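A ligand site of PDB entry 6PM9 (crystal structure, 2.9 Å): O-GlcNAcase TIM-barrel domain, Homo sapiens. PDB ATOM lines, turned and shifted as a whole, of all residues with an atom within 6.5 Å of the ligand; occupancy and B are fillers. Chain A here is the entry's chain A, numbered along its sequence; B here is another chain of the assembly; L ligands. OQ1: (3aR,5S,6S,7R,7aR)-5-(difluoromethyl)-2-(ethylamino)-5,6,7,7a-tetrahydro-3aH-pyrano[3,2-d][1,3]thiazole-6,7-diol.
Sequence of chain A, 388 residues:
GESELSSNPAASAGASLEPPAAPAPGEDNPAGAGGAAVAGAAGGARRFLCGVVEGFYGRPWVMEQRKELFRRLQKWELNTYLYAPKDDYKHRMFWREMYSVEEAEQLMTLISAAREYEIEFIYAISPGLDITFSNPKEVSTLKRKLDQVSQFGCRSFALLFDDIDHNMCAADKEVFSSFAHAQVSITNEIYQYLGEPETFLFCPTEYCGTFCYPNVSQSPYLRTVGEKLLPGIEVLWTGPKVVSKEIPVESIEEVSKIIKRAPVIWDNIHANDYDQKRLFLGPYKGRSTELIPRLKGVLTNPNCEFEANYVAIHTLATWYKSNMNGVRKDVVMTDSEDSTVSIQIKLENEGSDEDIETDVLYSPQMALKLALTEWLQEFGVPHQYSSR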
ATOM      1  N   GLY A  55      -8.232 -12.627  15.725  1.00  0.00           N
ATOM      2  CA  GLY A  55      -8.227 -12.877  14.289  1.00  0.00           C
ATOM      3  C   GLY A  55      -9.387 -12.336  13.475  1.00  0.00           C
ATOM      4  O   GLY A  55      -9.564 -12.697  12.308  1.00  0.00           O
ATOM      5  N   PHE A  56     -10.165 -11.482  14.095  1.00  0.00           N
ATOM      6  CA  PHE A  56     -11.303 -10.816  13.508  1.00  0.00           C
ATOM      7  C   PHE A  56     -10.847  -9.640  12.631  1.00  0.00           C
ATOM      8  O   PHE A  56      -9.678  -9.244  12.645  1.00  0.00           O
ATOM      9  CB  PHE A  56     -12.208 -10.266  14.646  1.00  0.00           C
ATOM     10  CG  PHE A  56     -11.496  -9.509  15.747  1.00  0.00           C
ATOM     11  CD1 PHE A  56     -11.086  -8.193  15.553  1.00  0.00           C
ATOM     12  CD2 PHE A  56     -11.239 -10.098  16.979  1.00  0.00           C
ATOM     13  CE1 PHE A  56     -10.426  -7.484  16.560  1.00  0.00           C
ATOM     14  CE2 PHE A  56     -10.585  -9.398  17.987  1.00  0.00           C
ATOM     15  CZ  PHE A  56     -10.182  -8.100  17.762  1.00  0.00           C
ATOM     16  N   TYR A  57     -11.772  -9.071  11.882  1.00  0.00           N
ATOM     17  CA  TYR A  57     -11.482  -7.898  11.078  1.00  0.00           C
ATOM     18  C   TYR A  57     -11.867  -6.716  11.974  1.00  0.00           C
ATOM     19  O   TYR A  57     -12.552  -6.884  12.987  1.00  0.00           O
ATOM     20  CB  TYR A  57     -12.331  -7.915   9.797  1.00  0.00           C
ATOM     21  CG  TYR A  57     -11.918  -8.983   8.797  1.00  0.00           C
ATOM     22  CD1 TYR A  57     -12.417 -10.278   8.880  1.00  0.00           C
ATOM     23  CD2 TYR A  57     -11.048  -8.683   7.746  1.00  0.00           C
ATOM     24  CE1 TYR A  57     -12.068 -11.259   7.948  1.00  0.00           C
ATOM     25  CE2 TYR A  57     -10.701  -9.651   6.803  1.00  0.00           C
ATOM     26  CZ  TYR A  57     -11.210 -10.939   6.905  1.00  0.00           C
ATOM     27  OH  TYR A  57     -10.852 -11.902   5.993  1.00  0.00           O
ATOM     28  N   ALA A  84      -3.255 -12.623  15.251  1.00  0.00           N
ATOM     29  CA  ALA A  84      -3.609 -12.623  13.842  1.00  0.00           C
ATOM     30  C   ALA A  84      -4.583 -11.471  13.506  1.00  0.00           C
ATOM     31  O   ALA A  84      -5.627 -11.715  12.902  1.00  0.00           O
ATOM     32  CB  ALA A  84      -4.228 -13.967  13.471  1.00  0.00           C
ATOM     33  N   LYS A  86      -6.288  -9.140  11.377  1.00  0.00           N
ATOM     34  CA  LYS A  86      -6.445  -8.955   9.918  1.00  0.00           C
ATOM     35  C   LYS A  86      -6.224  -7.539   9.405  1.00  0.00           C
ATOM     36  O   LYS A  86      -5.755  -7.363   8.277  1.00  0.00           O
ATOM     37  CB  LYS A  86      -7.818  -9.465   9.425  1.00  0.00           C
ATOM     38  CG  LYS A  86      -8.130 -10.917   9.749  1.00  0.00           C
ATOM     39  CD  LYS A  86      -8.232 -11.821   8.492  1.00  0.00           C
ATOM     40  CE  LYS A  86      -8.582 -13.249   8.851  1.00  0.00           C
ATOM     41  NZ  LYS A  86      -7.625 -13.864   9.838  1.00  0.00           N
ATOM     42  N   ASP A 162      -6.140 -18.328   4.904  1.00  0.00           N
ATOM     43  CA  ASP A 162      -7.571 -18.134   5.008  1.00  0.00           C
ATOM     44  C   ASP A 162      -7.991 -16.832   4.311  1.00  0.00           C
ATOM     45  O   ASP A 162      -7.243 -15.849   4.274  1.00  0.00           O
ATOM     46  CB  ASP A 162      -8.005 -18.111   6.512  1.00  0.00           C
ATOM     47  CG  ASP A 162      -7.355 -17.076   7.448  1.00  0.00           C
ATOM     48  OD1 ASP A 162      -6.146 -16.774   7.270  1.00  0.00           O
ATOM     49  OD2 ASP A 162      -8.043 -16.591   8.382  1.00  0.00           O
ATOM     50  N   ASP A 163      -9.203 -16.841   3.746  1.00  0.00           N
ATOM     51  CA  ASP A 163      -9.900 -15.766   3.061  1.00  0.00           C
ATOM     52  C   ASP A 163      -9.128 -15.212   1.823  1.00  0.00           C
ATOM     53  O   ASP A 163      -9.088 -14.004   1.565  1.00  0.00           O
ATOM     54  CB  ASP A 163     -10.308 -14.689   4.071  1.00  0.00           C
ATOM     55  CG  ASP A 163     -11.221 -15.234   5.173  1.00  0.00           C
ATOM     56  OD1 ASP A 163     -12.209 -15.967   4.836  1.00  0.00           O
ATOM     57  OD2 ASP A 163     -10.975 -14.928   6.361  1.00  0.00           O
ATOM     58  N   CYS A 203      -2.848 -22.508   8.636  1.00  0.00           N
ATOM     59  CA  CYS A 203      -4.269 -22.257   8.426  1.00  0.00           C
ATOM     60  C   CYS A 203      -4.678 -22.410   6.979  1.00  0.00           C
ATOM     61  O   CYS A 203      -4.239 -21.614   6.124  1.00  0.00           O
ATOM     62  CB  CYS A 203      -4.662 -20.902   8.988  1.00  0.00           C
ATOM     63  SG  CYS A 203      -6.431 -20.562   8.855  1.00  0.00           S
ATOM     64  N   PRO A 204      -5.536 -23.403   6.662  1.00  0.00           N
ATOM     65  CA  PRO A 204      -5.948 -23.625   5.260  1.00  0.00           C
ATOM     66  C   PRO A 204      -6.927 -22.621   4.650  1.00  0.00           C
ATOM     67  O   PRO A 204      -7.554 -21.805   5.369  1.00  0.00           O
ATOM     68  CB  PRO A 204      -6.566 -25.022   5.305  1.00  0.00           C
ATOM     69  CG  PRO A 204      -7.072 -25.177   6.700  1.00  0.00           C
ATOM     70  CD  PRO A 204      -6.121 -24.414   7.575  1.00  0.00           C
ATOM     71  N   TYR A 207     -10.959 -23.936   5.456  1.00  0.00           N
ATOM     72  CA  TYR A 207     -10.840 -23.954   6.921  1.00  0.00           C
ATOM     73  C   TYR A 207     -12.058 -24.410   7.721  1.00  0.00           C
ATOM     74  O   TYR A 207     -11.946 -24.553   8.941  1.00  0.00           O
ATOM     75  CB  TYR A 207     -10.362 -22.593   7.436  1.00  0.00           C
ATOM     76  CG  TYR A 207     -11.203 -21.383   7.091  1.00  0.00           C
ATOM     77  CD1 TYR A 207     -12.408 -21.136   7.751  1.00  0.00           C
ATOM     78  CD2 TYR A 207     -10.735 -20.416   6.209  1.00  0.00           C
ATOM     79  CE1 TYR A 207     -13.160 -19.995   7.480  1.00  0.00           C
ATOM     80  CE2 TYR A 207     -11.463 -19.255   5.949  1.00  0.00           C
ATOM     81  CZ  TYR A 207     -12.686 -19.043   6.579  1.00  0.00           C
ATOM     82  OH  TYR A 207     -13.439 -17.925   6.299  1.00  0.00           O
ATOM     83  N   LEU A 236      -5.445 -25.486  11.663  1.00  0.00           N
ATOM     84  CA  LEU A 236      -6.557 -24.765  12.274  1.00  0.00           C
ATOM     85  C   LEU A 236      -7.853 -25.133  11.550  1.00  0.00           C
ATOM     86  O   LEU A 236      -7.862 -25.281  10.328  1.00  0.00           O
ATOM     87  CB  LEU A 236      -6.285 -23.256  12.225  1.00  0.00           C
ATOM     88  CG  LEU A 236      -5.238 -22.733  13.205  1.00  0.00           C
ATOM     89  CD1 LEU A 236      -4.411 -21.629  12.585  1.00  0.00           C
ATOM     90  CD2 LEU A 236      -5.892 -22.213  14.463  1.00  0.00           C
ATOM     91  N   TRP A 237      -8.937 -25.330  12.310  1.00  0.00           N
ATOM     92  CA  TRP A 237     -10.246 -25.715  11.766  1.00  0.00           C
ATOM     93  C   TRP A 237     -11.378 -24.959  12.494  1.00  0.00           C
ATOM     94  O   TRP A 237     -11.364 -24.898  13.721  1.00  0.00           O
ATOM     95  CB  TRP A 237     -10.404 -27.238  11.869  1.00  0.00           C
ATOM     96  CG  TRP A 237     -11.521 -27.801  11.035  1.00  0.00           C
ATOM     97  CD1 TRP A 237     -12.694 -28.305  11.480  1.00  0.00           C
ATOM     98  CD2 TRP A 237     -11.541 -27.939   9.600  1.00  0.00           C
ATOM     99  NE1 TRP A 237     -13.457 -28.736  10.425  1.00  0.00           N
ATOM    100  CE2 TRP A 237     -12.773 -28.530   9.258  1.00  0.00           C
ATOM    101  CE3 TRP A 237     -10.627 -27.620   8.572  1.00  0.00           C
ATOM    102  CZ2 TRP A 237     -13.124 -28.791   7.925  1.00  0.00           C
ATOM    103  CZ3 TRP A 237     -10.978 -27.894   7.260  1.00  0.00           C
ATOM    104  CH2 TRP A 237     -12.216 -28.468   6.957  1.00  0.00           C
ATOM    105  N   THR A 238     -12.338 -24.368  11.759  1.00  0.00           N
ATOM    106  CA  THR A 238     -13.428 -23.637  12.423  1.00  0.00           C
ATOM    107  C   THR A 238     -14.683 -24.514  12.630  1.00  0.00           C
ATOM    108  O   THR A 238     -15.640 -24.069  13.265  1.00  0.00           O
ATOM    109  CB  THR A 238     -13.741 -22.250  11.773  1.00  0.00           C
ATOM    110  OG1 THR A 238     -14.591 -22.364  10.648  1.00  0.00           O
ATOM    111  CG2 THR A 238     -12.542 -21.502  11.386  1.00  0.00           C
ATOM    112  N   VAL A 242     -18.194 -21.431   9.232  1.00  0.00           N
ATOM    113  CA  VAL A 242     -17.269 -20.412   9.766  1.00  0.00           C
ATOM    114  C   VAL A 242     -17.662 -20.213  11.273  1.00  0.00           C
ATOM    115  O   VAL A 242     -16.851 -20.416  12.180  1.00  0.00           O
ATOM    116  CB  VAL A 242     -17.333 -19.109   8.926  1.00  0.00           C
ATOM    117  CG1 VAL A 242     -16.515 -18.011   9.555  1.00  0.00           C
ATOM    118  CG2 VAL A 242     -16.871 -19.351   7.500  1.00  0.00           C
ATOM    119  N   VAL A 243     -18.936 -19.871  11.507  1.00  0.00           N
ATOM    120  CA  VAL A 243     -19.505 -19.690  12.834  1.00  0.00           C
ATOM    121  C   VAL A 243     -20.324 -20.961  13.002  1.00  0.00           C
ATOM    122  O   VAL A 243     -21.416 -21.057  12.465  1.00  0.00           O
ATOM    123  CB  VAL A 243     -20.359 -18.405  12.907  1.00  0.00           C
ATOM    124  CG1 VAL A 243     -20.759 -18.083  14.335  1.00  0.00           C
ATOM    125  CG2 VAL A 243     -19.663 -17.217  12.237  1.00  0.00           C
ATOM    126  N   TRP A 266     -10.278 -22.870  15.655  1.00  0.00           N
ATOM    127  CA  TRP A 266     -10.261 -21.413  15.651  1.00  0.00           C
ATOM    128  C   TRP A 266     -11.768 -21.158  15.642  1.00  0.00           C
ATOM    129  O   TRP A 266     -12.381 -20.997  14.578  1.00  0.00           O
ATOM    130  CB  TRP A 266      -9.509 -20.812  14.428  1.00  0.00           C
ATOM    131  CG  TRP A 266      -9.709 -19.322  14.177  1.00  0.00           C
ATOM    132  CD1 TRP A 266     -10.875 -18.633  14.290  1.00  0.00           C
ATOM    133  CD2 TRP A 266      -8.734 -18.396  13.654  1.00  0.00           C
ATOM    134  NE1 TRP A 266     -10.693 -17.324  13.910  1.00  0.00           N
ATOM    135  CE2 TRP A 266      -9.390 -17.150  13.508  1.00  0.00           C
ATOM    136  CE3 TRP A 266      -7.381 -18.491  13.294  1.00  0.00           C
ATOM    137  CZ2 TRP A 266      -8.733 -15.999  13.028  1.00  0.00           C
ATOM    138  CZ3 TRP A 266      -6.731 -17.347  12.833  1.00  0.00           C
ATOM    139  CH2 TRP A 266      -7.405 -16.126  12.697  1.00  0.00           C
ATOM    140  N   ASN A 268     -15.397 -19.458  16.082  1.00  0.00           N
ATOM    141  CA  ASN A 268     -15.997 -18.140  15.787  1.00  0.00           C
ATOM    142  C   ASN A 268     -17.380 -17.993  16.413  1.00  0.00           C
ATOM    143  O   ASN A 268     -18.170 -17.134  15.993  1.00  0.00           O
ATOM    144  CB  ASN A 268     -16.022 -17.850  14.285  1.00  0.00           C
ATOM    145  CG  ASN A 268     -14.675 -17.678  13.657  1.00  0.00           C
ATOM    146  OD1 ASN A 268     -13.800 -17.006  14.176  1.00  0.00           O
ATOM    147  ND2 ASN A 268     -14.484 -18.284  12.504  1.00  0.00           N
ATOM    148  N   ILE A 269     -17.665 -18.805  17.447  1.00  0.00           N
ATOM    149  CA  ILE A 269     -18.922 -18.751  18.193  1.00  0.00           C
ATOM    150  C   ILE A 269     -19.226 -17.297  18.658  1.00  0.00           C
ATOM    151  O   ILE A 269     -20.288 -16.788  18.341  1.00  0.00           O
ATOM    152  CB  ILE A 269     -18.999 -19.814  19.326  1.00  0.00           C
ATOM    153  CG1 ILE A 269     -20.273 -19.656  20.155  1.00  0.00           C
ATOM    154  CG2 ILE A 269     -17.751 -19.820  20.229  1.00  0.00           C
ATOM    155  CD1 ILE A 269     -20.684 -20.859  20.927  1.00  0.00           C
ATOM    156  N   ALA A 271     -17.557 -14.485  17.656  1.00  0.00           N
ATOM    157  CA  ALA A 271     -17.032 -13.530  16.660  1.00  0.00           C
ATOM    158  C   ALA A 271     -18.152 -12.627  16.242  1.00  0.00           C
ATOM    159  O   ALA A 271     -19.265 -13.117  16.018  1.00  0.00           O
ATOM    160  CB  ALA A 271     -16.517 -14.281  15.440  1.00  0.00           C
ATOM    161  N   ASN A 272     -17.894 -11.322  16.142  1.00  0.00           N
ATOM    162  CA  ASN A 272     -18.950 -10.378  15.789  1.00  0.00           C
ATOM    163  C   ASN A 272     -18.544  -9.335  14.764  1.00  0.00           C
ATOM    164  O   ASN A 272     -19.247  -8.333  14.618  1.00  0.00           O
ATOM    165  CB  ASN A 272     -19.516  -9.713  17.069  1.00  0.00           C
ATOM    166  CG  ASN A 272     -18.810  -8.473  17.616  1.00  0.00           C
ATOM    167  OD1 ASN A 272     -17.644  -8.167  17.333  1.00  0.00           O
ATOM    168  ND2 ASN A 272     -19.521  -7.736  18.412  1.00  0.00           N
ATOM    169  N   ASP A 273     -17.433  -9.558  14.042  1.00  0.00           N
ATOM    170  CA  ASP A 273     -16.926  -8.638  13.015  1.00  0.00           C
ATOM    171  C   ASP A 273     -17.797  -8.535  11.755  1.00  0.00           C
ATOM    172  O   ASP A 273     -17.816  -7.488  11.127  1.00  0.00           O
ATOM    173  CB  ASP A 273     -15.475  -8.960  12.639  1.00  0.00           C
ATOM    174  CG  ASP A 273     -15.245 -10.379  12.174  1.00  0.00           C
ATOM    175  OD1 ASP A 273     -16.221 -11.146  12.093  1.00  0.00           O
ATOM    176  OD2 ASP A 273     -14.083 -10.721  11.888  1.00  0.00           O
ATOM    177  N   TYR A 274     -18.520  -9.625  11.408  1.00  0.00           N
ATOM    178  CA  TYR A 274     -19.399  -9.684  10.227  1.00  0.00           C
ATOM    179  C   TYR A 274     -20.745  -8.940  10.338  1.00  0.00           C
ATOM    180  O   TYR A 274     -21.607  -9.179   9.492  1.00  0.00           O
ATOM    181  CB  TYR A 274     -19.672 -11.141   9.860  1.00  0.00           C
ATOM    182  CG  TYR A 274     -20.230 -11.959  11.017  1.00  0.00           C
ATOM    183  CD1 TYR A 274     -21.561 -11.819  11.427  1.00  0.00           C
ATOM    184  CD2 TYR A 274     -19.439 -12.892  11.683  1.00  0.00           C
ATOM    185  CE1 TYR A 274     -22.078 -12.556  12.493  1.00  0.00           C
ATOM    186  CE2 TYR A 274     -19.956 -13.652  12.729  1.00  0.00           C
ATOM    187  CZ  TYR A 274     -21.271 -13.487  13.130  1.00  0.00           C
ATOM    188  OH  TYR A 274     -21.731 -14.236  14.172  1.00  0.00           O
ATOM    189  N   ASN A 301     -12.104 -16.882  18.758  1.00  0.00           N
ATOM    190  CA  ASN A 301     -12.013 -15.607  18.037  1.00  0.00           C
ATOM    191  C   ASN A 301     -13.269 -14.876  18.532  1.00  0.00           C
ATOM    192  O   ASN A 301     -14.372 -15.227  18.109  1.00  0.00           O
ATOM    193  CB  ASN A 301     -12.026 -15.844  16.538  1.00  0.00           C
ATOM    194  CG  ASN A 301     -11.784 -14.604  15.695  1.00  0.00           C
ATOM    195  OD1 ASN A 301     -11.055 -13.673  16.052  1.00  0.00           O
ATOM    196  ND2 ASN A 301     -12.395 -14.596  14.529  1.00  0.00           N
ATOM    197  N   PRO A 302     -13.148 -13.933  19.507  1.00  0.00           N
ATOM    198  CA  PRO A 302     -14.343 -13.313  20.085  1.00  0.00           C
ATOM    199  C   PRO A 302     -14.729 -11.950  19.498  1.00  0.00           C
ATOM    200  O   PRO A 302     -14.338 -11.653  18.365  1.00  0.00           O
ATOM    201  CB  PRO A 302     -13.979 -13.262  21.563  1.00  0.00           C
ATOM    202  CG  PRO A 302     -12.458 -13.064  21.566  1.00  0.00           C
ATOM    203  CD  PRO A 302     -11.943 -13.436  20.194  1.00  0.00           C
ATOM    204  N   TRP B 127     -24.663 -14.029   8.548  1.00  0.00           N
ATOM    205  CA  TRP B 127     -24.746 -12.797   7.771  1.00  0.00           C
ATOM    206  C   TRP B 127     -25.648 -13.090   6.551  1.00  0.00           C
ATOM    207  O   TRP B 127     -25.318 -13.929   5.720  1.00  0.00           O
ATOM    208  CB  TRP B 127     -23.342 -12.273   7.380  1.00  0.00           C
ATOM    209  CG  TRP B 127     -22.458 -13.263   6.668  1.00  0.00           C
ATOM    210  CD1 TRP B 127     -22.446 -13.554   5.337  1.00  0.00           C
ATOM    211  CD2 TRP B 127     -21.414 -14.060   7.253  1.00  0.00           C
ATOM    212  NE1 TRP B 127     -21.496 -14.507   5.064  1.00  0.00           N
ATOM    213  CE2 TRP B 127     -20.847 -14.834   6.222  1.00  0.00           C
ATOM    214  CE3 TRP B 127     -20.929 -14.214   8.565  1.00  0.00           C
ATOM    215  CZ2 TRP B 127     -19.785 -15.722   6.452  1.00  0.00           C
ATOM    216  CZ3 TRP B 127     -19.876 -15.096   8.793  1.00  0.00           C
ATOM    217  CH2 TRP B 127     -19.322 -15.838   7.749  1.00  0.00           C
HETATM  218  C1  OQ1 L   1     -13.576 -13.838  11.060  1.00  0.00           C
HETATM  219  C2  OQ1 L   1     -12.175 -14.223  10.581  1.00  0.00           C
HETATM  220  C3  OQ1 L   1     -12.155 -15.039   9.281  1.00  0.00           C
HETATM  221  C4  OQ1 L   1     -13.290 -16.037   9.287  1.00  0.00           C
HETATM  222  C5  OQ1 L   1     -15.985 -14.801  11.277  1.00  0.00           C
HETATM  223  C11 OQ1 L   1     -10.262 -19.184  10.420  1.00  0.00           C
HETATM  224  C9  OQ1 L   1     -11.049 -17.033   9.632  1.00  0.00           C
HETATM  225  C12 OQ1 L   1      -9.289 -20.196   9.911  1.00  0.00           C
HETATM  226  C   OQ1 L   1     -14.508 -15.047  11.050  1.00  0.00           C
HETATM  227  O   OQ1 L   1     -14.550 -15.552   9.725  1.00  0.00           O
HETATM  228  O6  OQ1 L   1     -11.414 -13.046  10.403  1.00  0.00           O
HETATM  229  O7  OQ1 L   1     -13.474 -13.277  12.378  1.00  0.00           O
HETATM  230  F   OQ1 L   1     -16.345 -15.071  12.564  1.00  0.00           F
HETATM  231  N   OQ1 L   1     -10.902 -15.796   9.262  1.00  0.00           N
HETATM  232  S   OQ1 L   1     -12.678 -17.532  10.037  1.00  0.00           S
HETATM  233  N10 OQ1 L   1     -10.003 -17.897   9.827  1.00  0.00           N
HETATM  234  F1  OQ1 L   1     -16.408 -13.571  10.855  1.00  0.00           F
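OD2 of Asp 163 lies close to N of the ligand (3.0 Å). Phe 56 touches the ligand. Tyr 57 touches the ligand (CE1 to O6, 3.1 Å). Lys 86 touches the ligand (CE to O6, 3.2 Å). Cys 203 touches the ligand. OH of Tyr 207 touches C4 of the ligand, at 3.5 Å. Thr 238 touches the ligand. CG1 of Val 242 touches O of the ligand, 3.2 Å away. Val 243 touches the ligand. CD2 of Trp 266 touches C11 of the ligand, 3.7 Å away. Ala 271 touches the ligand (CB to F, 3.0 Å). Tyr 274 touches the ligand. Hydrophobic or aromatic side chains that line the ligand: Phe 56, Tyr 57, Tyr 207, Val 242, Val 243, Trp 266, Ala 271 and Tyr 274. Along chain A the residues within 4 Å of the ligand span positions 55 to 301.
The side-chain amide nitrogen of Asn 268 lies close to a sulfur (S) of the ligand. The side-chain carboxylate (OD2) of Asp 273 lies within hydrogen-bond range of an oxygen (O7) of the ligand. The backbone carbonyl oxygen of Gly 55 sits at hydrogen-bond distance from an oxygen (O6) of the ligand (2.7 Å). OD2 of Asp 162 sits at hydrogen-bond distance from N10 of the ligand. ND2 of Asn 301 lies within hydrogen-bond range of O7 of the ligand (2.7 Å).
The side-chain amide oxygen of Asn 301 lies within hydrogen-bond range of the backbone NH of Gly 55 (3.0 Å). The backbone carbonyl oxygen (O) of Val 242 sits at hydrogen-bond distance from the side-chain hydroxyl (OG1) of Thr 238, at 3.4 Å. NZ of Lys 86 is in salt-bridge range of OD2 of Asp 162. N of Phe 56 is in hydrogen-bond range of OD1 of Asn 301 (3.1 Å). The side-chain carboxylate of Asp 163 lies within hydrogen-bond range of the side-chain hydroxyl of Tyr 207. OH of Tyr 57 is in hydrogen-bond range of OD2 of Asp 163. O of Gly 55 sits at hydrogen-bond distance from NZ of Lys 86 (3.4 Å). The side-chain amide nitrogen (ND2) of Asn 301 lies close to the indole nitrogen (NE1) of Trp 266.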
